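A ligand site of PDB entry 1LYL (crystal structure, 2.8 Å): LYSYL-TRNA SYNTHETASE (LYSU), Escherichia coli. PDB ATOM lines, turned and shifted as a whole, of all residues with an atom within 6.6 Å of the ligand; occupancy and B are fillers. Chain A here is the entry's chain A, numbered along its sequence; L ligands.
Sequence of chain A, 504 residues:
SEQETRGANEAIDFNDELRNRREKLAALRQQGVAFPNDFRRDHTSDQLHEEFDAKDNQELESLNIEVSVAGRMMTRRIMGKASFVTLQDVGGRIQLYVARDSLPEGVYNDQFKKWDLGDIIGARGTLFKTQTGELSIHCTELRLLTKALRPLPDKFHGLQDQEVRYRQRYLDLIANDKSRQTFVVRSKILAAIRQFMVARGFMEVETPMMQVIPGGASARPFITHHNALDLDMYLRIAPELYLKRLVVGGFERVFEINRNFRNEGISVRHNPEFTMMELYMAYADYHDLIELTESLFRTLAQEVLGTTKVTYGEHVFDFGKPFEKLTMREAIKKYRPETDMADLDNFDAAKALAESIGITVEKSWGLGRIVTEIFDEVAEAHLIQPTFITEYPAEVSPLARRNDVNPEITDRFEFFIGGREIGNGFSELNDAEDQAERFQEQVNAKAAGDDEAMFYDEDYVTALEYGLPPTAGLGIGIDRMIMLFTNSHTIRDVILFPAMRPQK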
ATOM      1  N   GLY A 215     -29.146 -16.430   4.069  1.00  0.00           N
ATOM      2  CA  GLY A 215     -27.763 -16.568   3.636  1.00  0.00           C
ATOM      3  C   GLY A 215     -26.991 -17.527   4.511  1.00  0.00           C
ATOM      4  O   GLY A 215     -27.544 -18.135   5.424  1.00  0.00           O
ATOM      5  N   GLY A 216     -25.690 -17.648   4.234  1.00  0.00           N
ATOM      6  CA  GLY A 216     -24.860 -18.537   5.003  1.00  0.00           C
ATOM      7  C   GLY A 216     -24.711 -19.917   4.377  1.00  0.00           C
ATOM      8  O   GLY A 216     -23.934 -20.754   4.857  1.00  0.00           O
ATOM      9  N   ALA A 217     -25.435 -20.143   3.281  1.00  0.00           N
ATOM     10  CA  ALA A 217     -25.369 -21.419   2.577  1.00  0.00           C
ATOM     11  C   ALA A 217     -26.155 -21.309   1.289  1.00  0.00           C
ATOM     12  O   ALA A 217     -26.783 -20.291   1.021  1.00  0.00           O
ATOM     13  CB  ALA A 217     -25.941 -22.541   3.443  1.00  0.00           C
ATOM     14  N   ILE A 237     -31.569 -20.371   6.773  1.00  0.00           N
ATOM     15  CA  ILE A 237     -30.943 -21.535   6.167  1.00  0.00           C
ATOM     16  C   ILE A 237     -29.567 -21.764   6.783  1.00  0.00           C
ATOM     17  O   ILE A 237     -28.972 -22.823   6.625  1.00  0.00           O
ATOM     18  CB  ILE A 237     -30.798 -21.439   4.629  1.00  0.00           C
ATOM     19  CG1 ILE A 237     -29.962 -20.252   4.219  1.00  0.00           C
ATOM     20  CG2 ILE A 237     -32.162 -21.387   3.971  1.00  0.00           C
ATOM     21  CD1 ILE A 237     -29.752 -20.188   2.715  1.00  0.00           C
ATOM     22  N   ALA A 238     -29.083 -20.764   7.526  1.00  0.00           N
ATOM     23  CA  ALA A 238     -27.814 -20.819   8.256  1.00  0.00           C
ATOM     24  C   ALA A 238     -27.663 -19.530   9.064  1.00  0.00           C
ATOM     25  O   ALA A 238     -28.018 -18.457   8.574  1.00  0.00           O
ATOM     26  CB  ALA A 238     -26.667 -20.951   7.306  1.00  0.00           C
ATOM     27  N   PRO A 239     -27.153 -19.618  10.313  1.00  0.00           N
ATOM     28  CA  PRO A 239     -26.958 -18.447  11.176  1.00  0.00           C
ATOM     29  C   PRO A 239     -25.604 -17.745  10.961  1.00  0.00           C
ATOM     30  O   PRO A 239     -25.229 -16.855  11.745  1.00  0.00           O
ATOM     31  CB  PRO A 239     -26.997 -19.076  12.550  1.00  0.00           C
ATOM     32  CG  PRO A 239     -26.197 -20.367  12.298  1.00  0.00           C
ATOM     33  CD  PRO A 239     -26.927 -20.864  11.070  1.00  0.00           C
ATOM     34  N   GLU A 240     -24.909 -18.089   9.882  1.00  0.00           N
ATOM     35  CA  GLU A 240     -23.523 -17.644   9.666  1.00  0.00           C
ATOM     36  C   GLU A 240     -23.271 -16.141   9.661  1.00  0.00           C
ATOM     37  O   GLU A 240     -22.459 -15.649  10.445  1.00  0.00           O
ATOM     38  CB  GLU A 240     -22.949 -18.251   8.393  1.00  0.00           C
ATOM     39  CG  GLU A 240     -21.559 -17.717   8.040  1.00  0.00           C
ATOM     40  CD  GLU A 240     -20.844 -18.527   6.963  1.00  0.00           C
ATOM     41  OE1 GLU A 240     -21.290 -19.653   6.632  1.00  0.00           O
ATOM     42  OE2 GLU A 240     -19.833 -18.034   6.446  1.00  0.00           O
ATOM     43  N   LYS A 244     -21.081 -14.023  12.496  1.00  0.00           N
ATOM     44  CA  LYS A 244     -19.880 -13.276  12.151  1.00  0.00           C
ATOM     45  C   LYS A 244     -20.016 -11.801  12.499  1.00  0.00           C
ATOM     46  O   LYS A 244     -19.035 -11.133  12.860  1.00  0.00           O
ATOM     47  CB  LYS A 244     -19.504 -13.477  10.685  1.00  0.00           C
ATOM     48  CG  LYS A 244     -18.291 -14.379  10.498  1.00  0.00           C
ATOM     49  CD  LYS A 244     -17.899 -14.535   9.027  1.00  0.00           C
ATOM     50  CE  LYS A 244     -18.841 -15.473   8.279  1.00  0.00           C
ATOM     51  NZ  LYS A 244     -18.435 -15.637   6.858  1.00  0.00           N
ATOM     52  N   ASN A 260     -31.893 -25.222  11.337  1.00  0.00           N
ATOM     53  CA  ASN A 260     -31.852 -24.561  10.041  1.00  0.00           C
ATOM     54  C   ASN A 260     -33.016 -25.156   9.272  1.00  0.00           C
ATOM     55  O   ASN A 260     -33.463 -26.263   9.600  1.00  0.00           O
ATOM     56  CB  ASN A 260     -30.566 -24.874   9.285  1.00  0.00           C
ATOM     57  CG  ASN A 260     -29.349 -24.209   9.871  1.00  0.00           C
ATOM     58  OD1 ASN A 260     -29.421 -23.464  10.858  1.00  0.00           O
ATOM     59  ND2 ASN A 260     -28.198 -24.466   9.272  1.00  0.00           N
ATOM     60  N   ARG A 262     -34.635 -25.922   5.253  1.00  0.00           N
ATOM     61  CA  ARG A 262     -34.377 -26.011   3.812  1.00  0.00           C
ATOM     62  C   ARG A 262     -35.486 -26.761   3.083  1.00  0.00           C
ATOM     63  O   ARG A 262     -35.960 -27.789   3.554  1.00  0.00           O
ATOM     64  CB  ARG A 262     -33.036 -26.703   3.557  1.00  0.00           C
ATOM     65  CG  ARG A 262     -31.870 -25.928   4.129  1.00  0.00           C
ATOM     66  CD  ARG A 262     -30.516 -26.548   3.859  1.00  0.00           C
ATOM     67  NE  ARG A 262     -29.486 -25.881   4.671  1.00  0.00           N
ATOM     68  CZ  ARG A 262     -28.183 -25.984   4.456  1.00  0.00           C
ATOM     69  NH1 ARG A 262     -27.723 -26.705   3.441  1.00  0.00           N
ATOM     70  NH2 ARG A 262     -27.319 -25.372   5.273  1.00  0.00           N
ATOM     71  N   MET A 276     -28.008 -27.820  13.520  1.00  0.00           N
ATOM     72  CA  MET A 276     -26.642 -27.516  13.118  1.00  0.00           C
ATOM     73  C   MET A 276     -25.961 -26.774  14.246  1.00  0.00           C
ATOM     74  O   MET A 276     -26.612 -26.094  15.046  1.00  0.00           O
ATOM     75  CB  MET A 276     -26.618 -26.604  11.895  1.00  0.00           C
ATOM     76  CG  MET A 276     -26.918 -27.268  10.555  1.00  0.00           C
ATOM     77  SD  MET A 276     -25.483 -28.104   9.852  1.00  0.00           S
ATOM     78  CE  MET A 276     -24.466 -26.746   9.343  1.00  0.00           C
ATOM     79  N   MET A 277     -24.647 -26.910  14.320  1.00  0.00           N
ATOM     80  CA  MET A 277     -23.858 -26.148  15.260  1.00  0.00           C
ATOM     81  C   MET A 277     -22.882 -25.365  14.432  1.00  0.00           C
ATOM     82  O   MET A 277     -22.292 -25.906  13.499  1.00  0.00           O
ATOM     83  CB  MET A 277     -23.085 -27.052  16.212  1.00  0.00           C
ATOM     84  CG  MET A 277     -21.956 -26.328  16.929  1.00  0.00           C
ATOM     85  SD  MET A 277     -21.217 -27.239  18.284  1.00  0.00           S
ATOM     86  CE  MET A 277     -19.771 -27.889  17.526  1.00  0.00           C
ATOM     87  N   GLU A 278     -22.722 -24.086  14.746  1.00  0.00           N
ATOM     88  CA  GLU A 278     -21.696 -23.271  14.110  1.00  0.00           C
ATOM     89  C   GLU A 278     -20.878 -22.623  15.196  1.00  0.00           C
ATOM     90  O   GLU A 278     -21.389 -22.321  16.272  1.00  0.00           O
ATOM     91  CB  GLU A 278     -22.309 -22.205  13.208  1.00  0.00           C
ATOM     92  CG  GLU A 278     -22.973 -22.761  11.971  1.00  0.00           C
ATOM     93  CD  GLU A 278     -23.083 -21.716  10.881  1.00  0.00           C
ATOM     94  OE1 GLU A 278     -22.239 -20.790  10.862  1.00  0.00           O
ATOM     95  OE2 GLU A 278     -24.003 -21.812  10.042  1.00  0.00           O
ATOM     96  N   LEU A 279     -19.593 -22.447  14.934  1.00  0.00           N
ATOM     97  CA  LEU A 279     -18.688 -21.843  15.906  1.00  0.00           C
ATOM     98  C   LEU A 279     -17.683 -20.999  15.144  1.00  0.00           C
ATOM     99  O   LEU A 279     -17.303 -21.343  14.020  1.00  0.00           O
ATOM    100  CB  LEU A 279     -17.970 -22.925  16.704  1.00  0.00           C
ATOM    101  CG  LEU A 279     -17.035 -23.844  15.919  1.00  0.00           C
ATOM    102  CD1 LEU A 279     -15.584 -23.398  16.099  1.00  0.00           C
ATOM    103  CD2 LEU A 279     -17.194 -25.257  16.396  1.00  0.00           C
ATOM    104  N   TYR A 280     -17.280 -19.873  15.729  1.00  0.00           N
ATOM    105  CA  TYR A 280     -16.310 -18.991  15.105  1.00  0.00           C
ATOM    106  C   TYR A 280     -15.321 -18.603  16.164  1.00  0.00           C
ATOM    107  O   TYR A 280     -15.714 -18.248  17.261  1.00  0.00           O
ATOM    108  CB  TYR A 280     -16.986 -17.749  14.553  1.00  0.00           C
ATOM    109  CG  TYR A 280     -17.909 -18.042  13.406  1.00  0.00           C
ATOM    110  CD1 TYR A 280     -19.191 -18.526  13.628  1.00  0.00           C
ATOM    111  CD2 TYR A 280     -17.459 -17.934  12.092  1.00  0.00           C
ATOM    112  CE1 TYR A 280     -20.001 -18.893  12.570  1.00  0.00           C
ATOM    113  CE2 TYR A 280     -18.269 -18.305  11.043  1.00  0.00           C
ATOM    114  CZ  TYR A 280     -19.539 -18.786  11.287  1.00  0.00           C
ATOM    115  OH  TYR A 280     -20.322 -19.226  10.250  1.00  0.00           O
ATOM    116  N   LEU A 289      -9.226 -25.481  13.134  1.00  0.00           N
ATOM    117  CA  LEU A 289     -10.539 -26.108  13.148  1.00  0.00           C
ATOM    118  C   LEU A 289     -10.420 -27.622  12.970  1.00  0.00           C
ATOM    119  O   LEU A 289     -11.170 -28.383  13.569  1.00  0.00           O
ATOM    120  CB  LEU A 289     -11.425 -25.527  12.042  1.00  0.00           C
ATOM    121  CG  LEU A 289     -11.813 -24.056  12.207  1.00  0.00           C
ATOM    122  CD1 LEU A 289     -12.686 -23.652  11.060  1.00  0.00           C
ATOM    123  CD2 LEU A 289     -12.543 -23.825  13.526  1.00  0.00           C
ATOM    124  N   LEU A 399     -17.854 -17.243   0.875  1.00  0.00           N
ATOM    125  CA  LEU A 399     -17.580 -16.651   2.176  1.00  0.00           C
ATOM    126  C   LEU A 399     -16.249 -17.061   2.777  1.00  0.00           C
ATOM    127  O   LEU A 399     -15.988 -16.781   3.940  1.00  0.00           O
ATOM    128  CB  LEU A 399     -18.693 -17.013   3.170  1.00  0.00           C
ATOM    129  CG  LEU A 399     -20.120 -16.631   2.752  1.00  0.00           C
ATOM    130  CD1 LEU A 399     -21.127 -17.459   3.500  1.00  0.00           C
ATOM    131  CD2 LEU A 399     -20.383 -15.153   2.994  1.00  0.00           C
ATOM    132  N   GLU A 421     -21.311 -36.012   4.147  1.00  0.00           N
ATOM    133  CA  GLU A 421     -20.702 -34.780   4.636  1.00  0.00           C
ATOM    134  C   GLU A 421     -21.151 -34.466   6.058  1.00  0.00           C
ATOM    135  O   GLU A 421     -22.316 -34.206   6.281  1.00  0.00           O
ATOM    136  CB  GLU A 421     -21.112 -33.629   3.717  1.00  0.00           C
ATOM    137  CG  GLU A 421     -20.647 -32.258   4.191  1.00  0.00           C
ATOM    138  CD  GLU A 421     -21.495 -31.116   3.647  1.00  0.00           C
ATOM    139  OE1 GLU A 421     -22.010 -31.237   2.509  1.00  0.00           O
ATOM    140  OE2 GLU A 421     -21.638 -30.099   4.362  1.00  0.00           O
ATOM    141  N   ASN A 424     -18.200 -28.671   7.679  1.00  0.00           N
ATOM    142  CA  ASN A 424     -17.775 -27.712   6.662  1.00  0.00           C
ATOM    143  C   ASN A 424     -17.245 -26.517   7.437  1.00  0.00           C
ATOM    144  O   ASN A 424     -17.938 -26.002   8.315  1.00  0.00           O
ATOM    145  CB  ASN A 424     -18.990 -27.290   5.839  1.00  0.00           C
ATOM    146  CG  ASN A 424     -18.717 -26.102   4.953  1.00  0.00           C
ATOM    147  OD1 ASN A 424     -17.629 -25.950   4.408  1.00  0.00           O
ATOM    148  ND2 ASN A 424     -19.725 -25.268   4.788  1.00  0.00           N
ATOM    149  N   GLY A 425     -16.021 -26.119   7.153  1.00  0.00           N
ATOM    150  CA  GLY A 425     -15.436 -25.012   7.887  1.00  0.00           C
ATOM    151  C   GLY A 425     -14.370 -24.342   7.057  1.00  0.00           C
ATOM    152  O   GLY A 425     -13.913 -24.896   6.057  1.00  0.00           O
ATOM    153  N   PHE A 426     -13.955 -23.151   7.462  1.00  0.00           N
ATOM    154  CA  PHE A 426     -12.926 -22.446   6.726  1.00  0.00           C
ATOM    155  C   PHE A 426     -12.411 -21.185   7.367  1.00  0.00           C
ATOM    156  O   PHE A 426     -12.974 -20.687   8.355  1.00  0.00           O
ATOM    157  CB  PHE A 426     -13.386 -22.131   5.305  1.00  0.00           C
ATOM    158  CG  PHE A 426     -14.753 -21.505   5.221  1.00  0.00           C
ATOM    159  CD1 PHE A 426     -14.936 -20.141   5.463  1.00  0.00           C
ATOM    160  CD2 PHE A 426     -15.849 -22.257   4.836  1.00  0.00           C
ATOM    161  CE1 PHE A 426     -16.194 -19.546   5.311  1.00  0.00           C
ATOM    162  CE2 PHE A 426     -17.106 -21.680   4.677  1.00  0.00           C
ATOM    163  CZ  PHE A 426     -17.279 -20.325   4.915  1.00  0.00           C
ATOM    164  N   SER A 427     -11.300 -20.702   6.836  1.00  0.00           N
ATOM    165  CA  SER A 427     -10.731 -19.431   7.225  1.00  0.00           C
ATOM    166  C   SER A 427     -11.693 -18.446   6.575  1.00  0.00           C
ATOM    167  O   SER A 427     -11.916 -18.506   5.357  1.00  0.00           O
ATOM    168  CB  SER A 427      -9.324 -19.275   6.639  1.00  0.00           C
ATOM    169  OG  SER A 427      -8.450 -20.247   7.195  1.00  0.00           O
ATOM    170  N   GLU A 428     -12.297 -17.599   7.395  1.00  0.00           N
ATOM    171  CA  GLU A 428     -13.331 -16.665   6.959  1.00  0.00           C
ATOM    172  C   GLU A 428     -12.821 -15.511   6.112  1.00  0.00           C
ATOM    173  O   GLU A 428     -11.735 -14.982   6.352  1.00  0.00           O
ATOM    174  CB  GLU A 428     -14.026 -16.099   8.183  1.00  0.00           C
ATOM    175  CG  GLU A 428     -14.538 -17.152   9.126  1.00  0.00           C
ATOM    176  CD  GLU A 428     -15.714 -17.933   8.564  1.00  0.00           C
ATOM    177  OE1 GLU A 428     -16.368 -17.459   7.619  1.00  0.00           O
ATOM    178  OE2 GLU A 428     -15.987 -19.023   9.110  1.00  0.00           O
ATOM    179  N   ALA A 472     -11.774 -18.173  11.971  1.00  0.00           N
ATOM    180  CA  ALA A 472     -12.018 -19.490  11.400  1.00  0.00           C
ATOM    181  C   ALA A 472     -13.362 -19.963  11.926  1.00  0.00           C
ATOM    182  O   ALA A 472     -13.658 -19.840  13.124  1.00  0.00           O
ATOM    183  CB  ALA A 472     -10.943 -20.439  11.826  1.00  0.00           C
ATOM    184  N   GLY A 473     -14.199 -20.478  11.037  1.00  0.00           N
ATOM    185  CA  GLY A 473     -15.512 -20.921  11.442  1.00  0.00           C
ATOM    186  C   GLY A 473     -15.794 -22.321  10.960  1.00  0.00           C
ATOM    187  O   GLY A 473     -15.314 -22.729   9.898  1.00  0.00           O
ATOM    188  N   LEU A 474     -16.608 -23.045  11.721  1.00  0.00           N
ATOM    189  CA  LEU A 474     -16.919 -24.439  11.429  1.00  0.00           C
ATOM    190  C   LEU A 474     -18.387 -24.727  11.674  1.00  0.00           C
ATOM    191  O   LEU A 474     -18.972 -24.223  12.645  1.00  0.00           O
ATOM    192  CB  LEU A 474     -16.069 -25.330  12.335  1.00  0.00           C
ATOM    193  CG  LEU A 474     -16.276 -26.840  12.257  1.00  0.00           C
ATOM    194  CD1 LEU A 474     -15.899 -27.323  10.892  1.00  0.00           C
ATOM    195  CD2 LEU A 474     -15.426 -27.519  13.305  1.00  0.00           C
ATOM    196  N   GLY A 475     -18.987 -25.526  10.797  1.00  0.00           N
ATOM    197  CA  GLY A 475     -20.359 -25.937  10.960  1.00  0.00           C
ATOM    198  C   GLY A 475     -20.398 -27.452  10.971  1.00  0.00           C
ATOM    199  O   GLY A 475     -19.720 -28.098  10.172  1.00  0.00           O
ATOM    200  N   ILE A 476     -21.164 -28.040  11.881  1.00  0.00           N
ATOM    201  CA  ILE A 476     -21.242 -29.487  12.010  1.00  0.00           C
ATOM    202  C   ILE A 476     -22.696 -29.943  12.087  1.00  0.00           C
ATOM    203  O   ILE A 476     -23.453 -29.419  12.910  1.00  0.00           O
ATOM    204  CB  ILE A 476     -20.487 -29.957  13.273  1.00  0.00           C
ATOM    205  CG1 ILE A 476     -18.989 -29.704  13.141  1.00  0.00           C
ATOM    206  CG2 ILE A 476     -20.757 -31.408  13.540  1.00  0.00           C
ATOM    207  CD1 ILE A 476     -18.194 -30.240  14.307  1.00  0.00           C
HETATM  208  N1  LIG L   1     -23.126 -22.270   7.259  1.00  0.00           N
HETATM  209  C1  LIG L   1     -22.126 -23.180   6.721  1.00  0.00           C
HETATM  210  C2  LIG L   1     -22.814 -24.286   5.944  1.00  0.00           C
HETATM  211  O1  LIG L   1     -23.853 -24.761   6.362  1.00  0.00           O
HETATM  212  C3  LIG L   1     -21.325 -23.803   7.862  1.00  0.00           C
HETATM  213  C4  LIG L   1     -20.438 -22.826   8.587  1.00  0.00           C
HETATM  214  C5  LIG L   1     -19.185 -22.536   7.811  1.00  0.00           C
HETATM  215  C6  LIG L   1     -18.658 -21.163   8.160  1.00  0.00           C
HETATM  216  N2  LIG L   1     -17.208 -21.204   8.129  1.00  0.00           N
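OE1 of Glu 240 lies within salt-bridge range of N1 of the ligand (3.3 Å). O of Gly 473 is in hydrogen-bond range of N2 of the ligand (3.0 Å). A nitrogen (N1) of the ligand is in hydrogen-bond range of the backbone carbonyl oxygen (O) of Gly 216 (3.0 Å). The side-chain carboxylate (OE2) of Glu 278 is in salt-bridge range of a nitrogen (N1) of the ligand (3.0 Å). OE2 of Glu 428 is in salt-bridge range of N2 of the ligand, at 2.7 Å.
The backbone NH of Phe 426 is in hydrogen-bond range of the backbone carbonyl oxygen of Gly 473 (2.8 Å). The guanidinium group of Arg 262 sits at hydrogen-bond distance from the backbone carbonyl oxygen of Ile 237. NZ of Lys 244 lies within salt-bridge range of OE1 of Glu 428 (2.9 Å). OE2 of Glu 428 sits at hydrogen-bond distance from N of Gly 473, at 3.0 Å. The side-chain hydroxyl (OH) of Tyr 280 lies within hydrogen-bond range of the side-chain carboxylate (OE1) of Glu 278, at 2.5 Å. N of Gly 475 sits at hydrogen-bond distance from O of Asn 424 (2.7 Å). OE2 of Glu 240 lies within salt-bridge range of NZ of Lys 244 (2.8 Å).
CB of Ala 238 touches N1 of the ligand (3.8 Å). Arg 262 touches the ligand (NH2 to O1, 3.7 Å). Met 276 touches the ligand (CE to O1, 3.6 Å). Tyr 280 touches the ligand (OH to C6, 3.3 Å). Asn 424 touches the ligand. CZ of Phe 426 touches N2 of the ligand, at 3.3 Å. Gly 475 touches the ligand.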
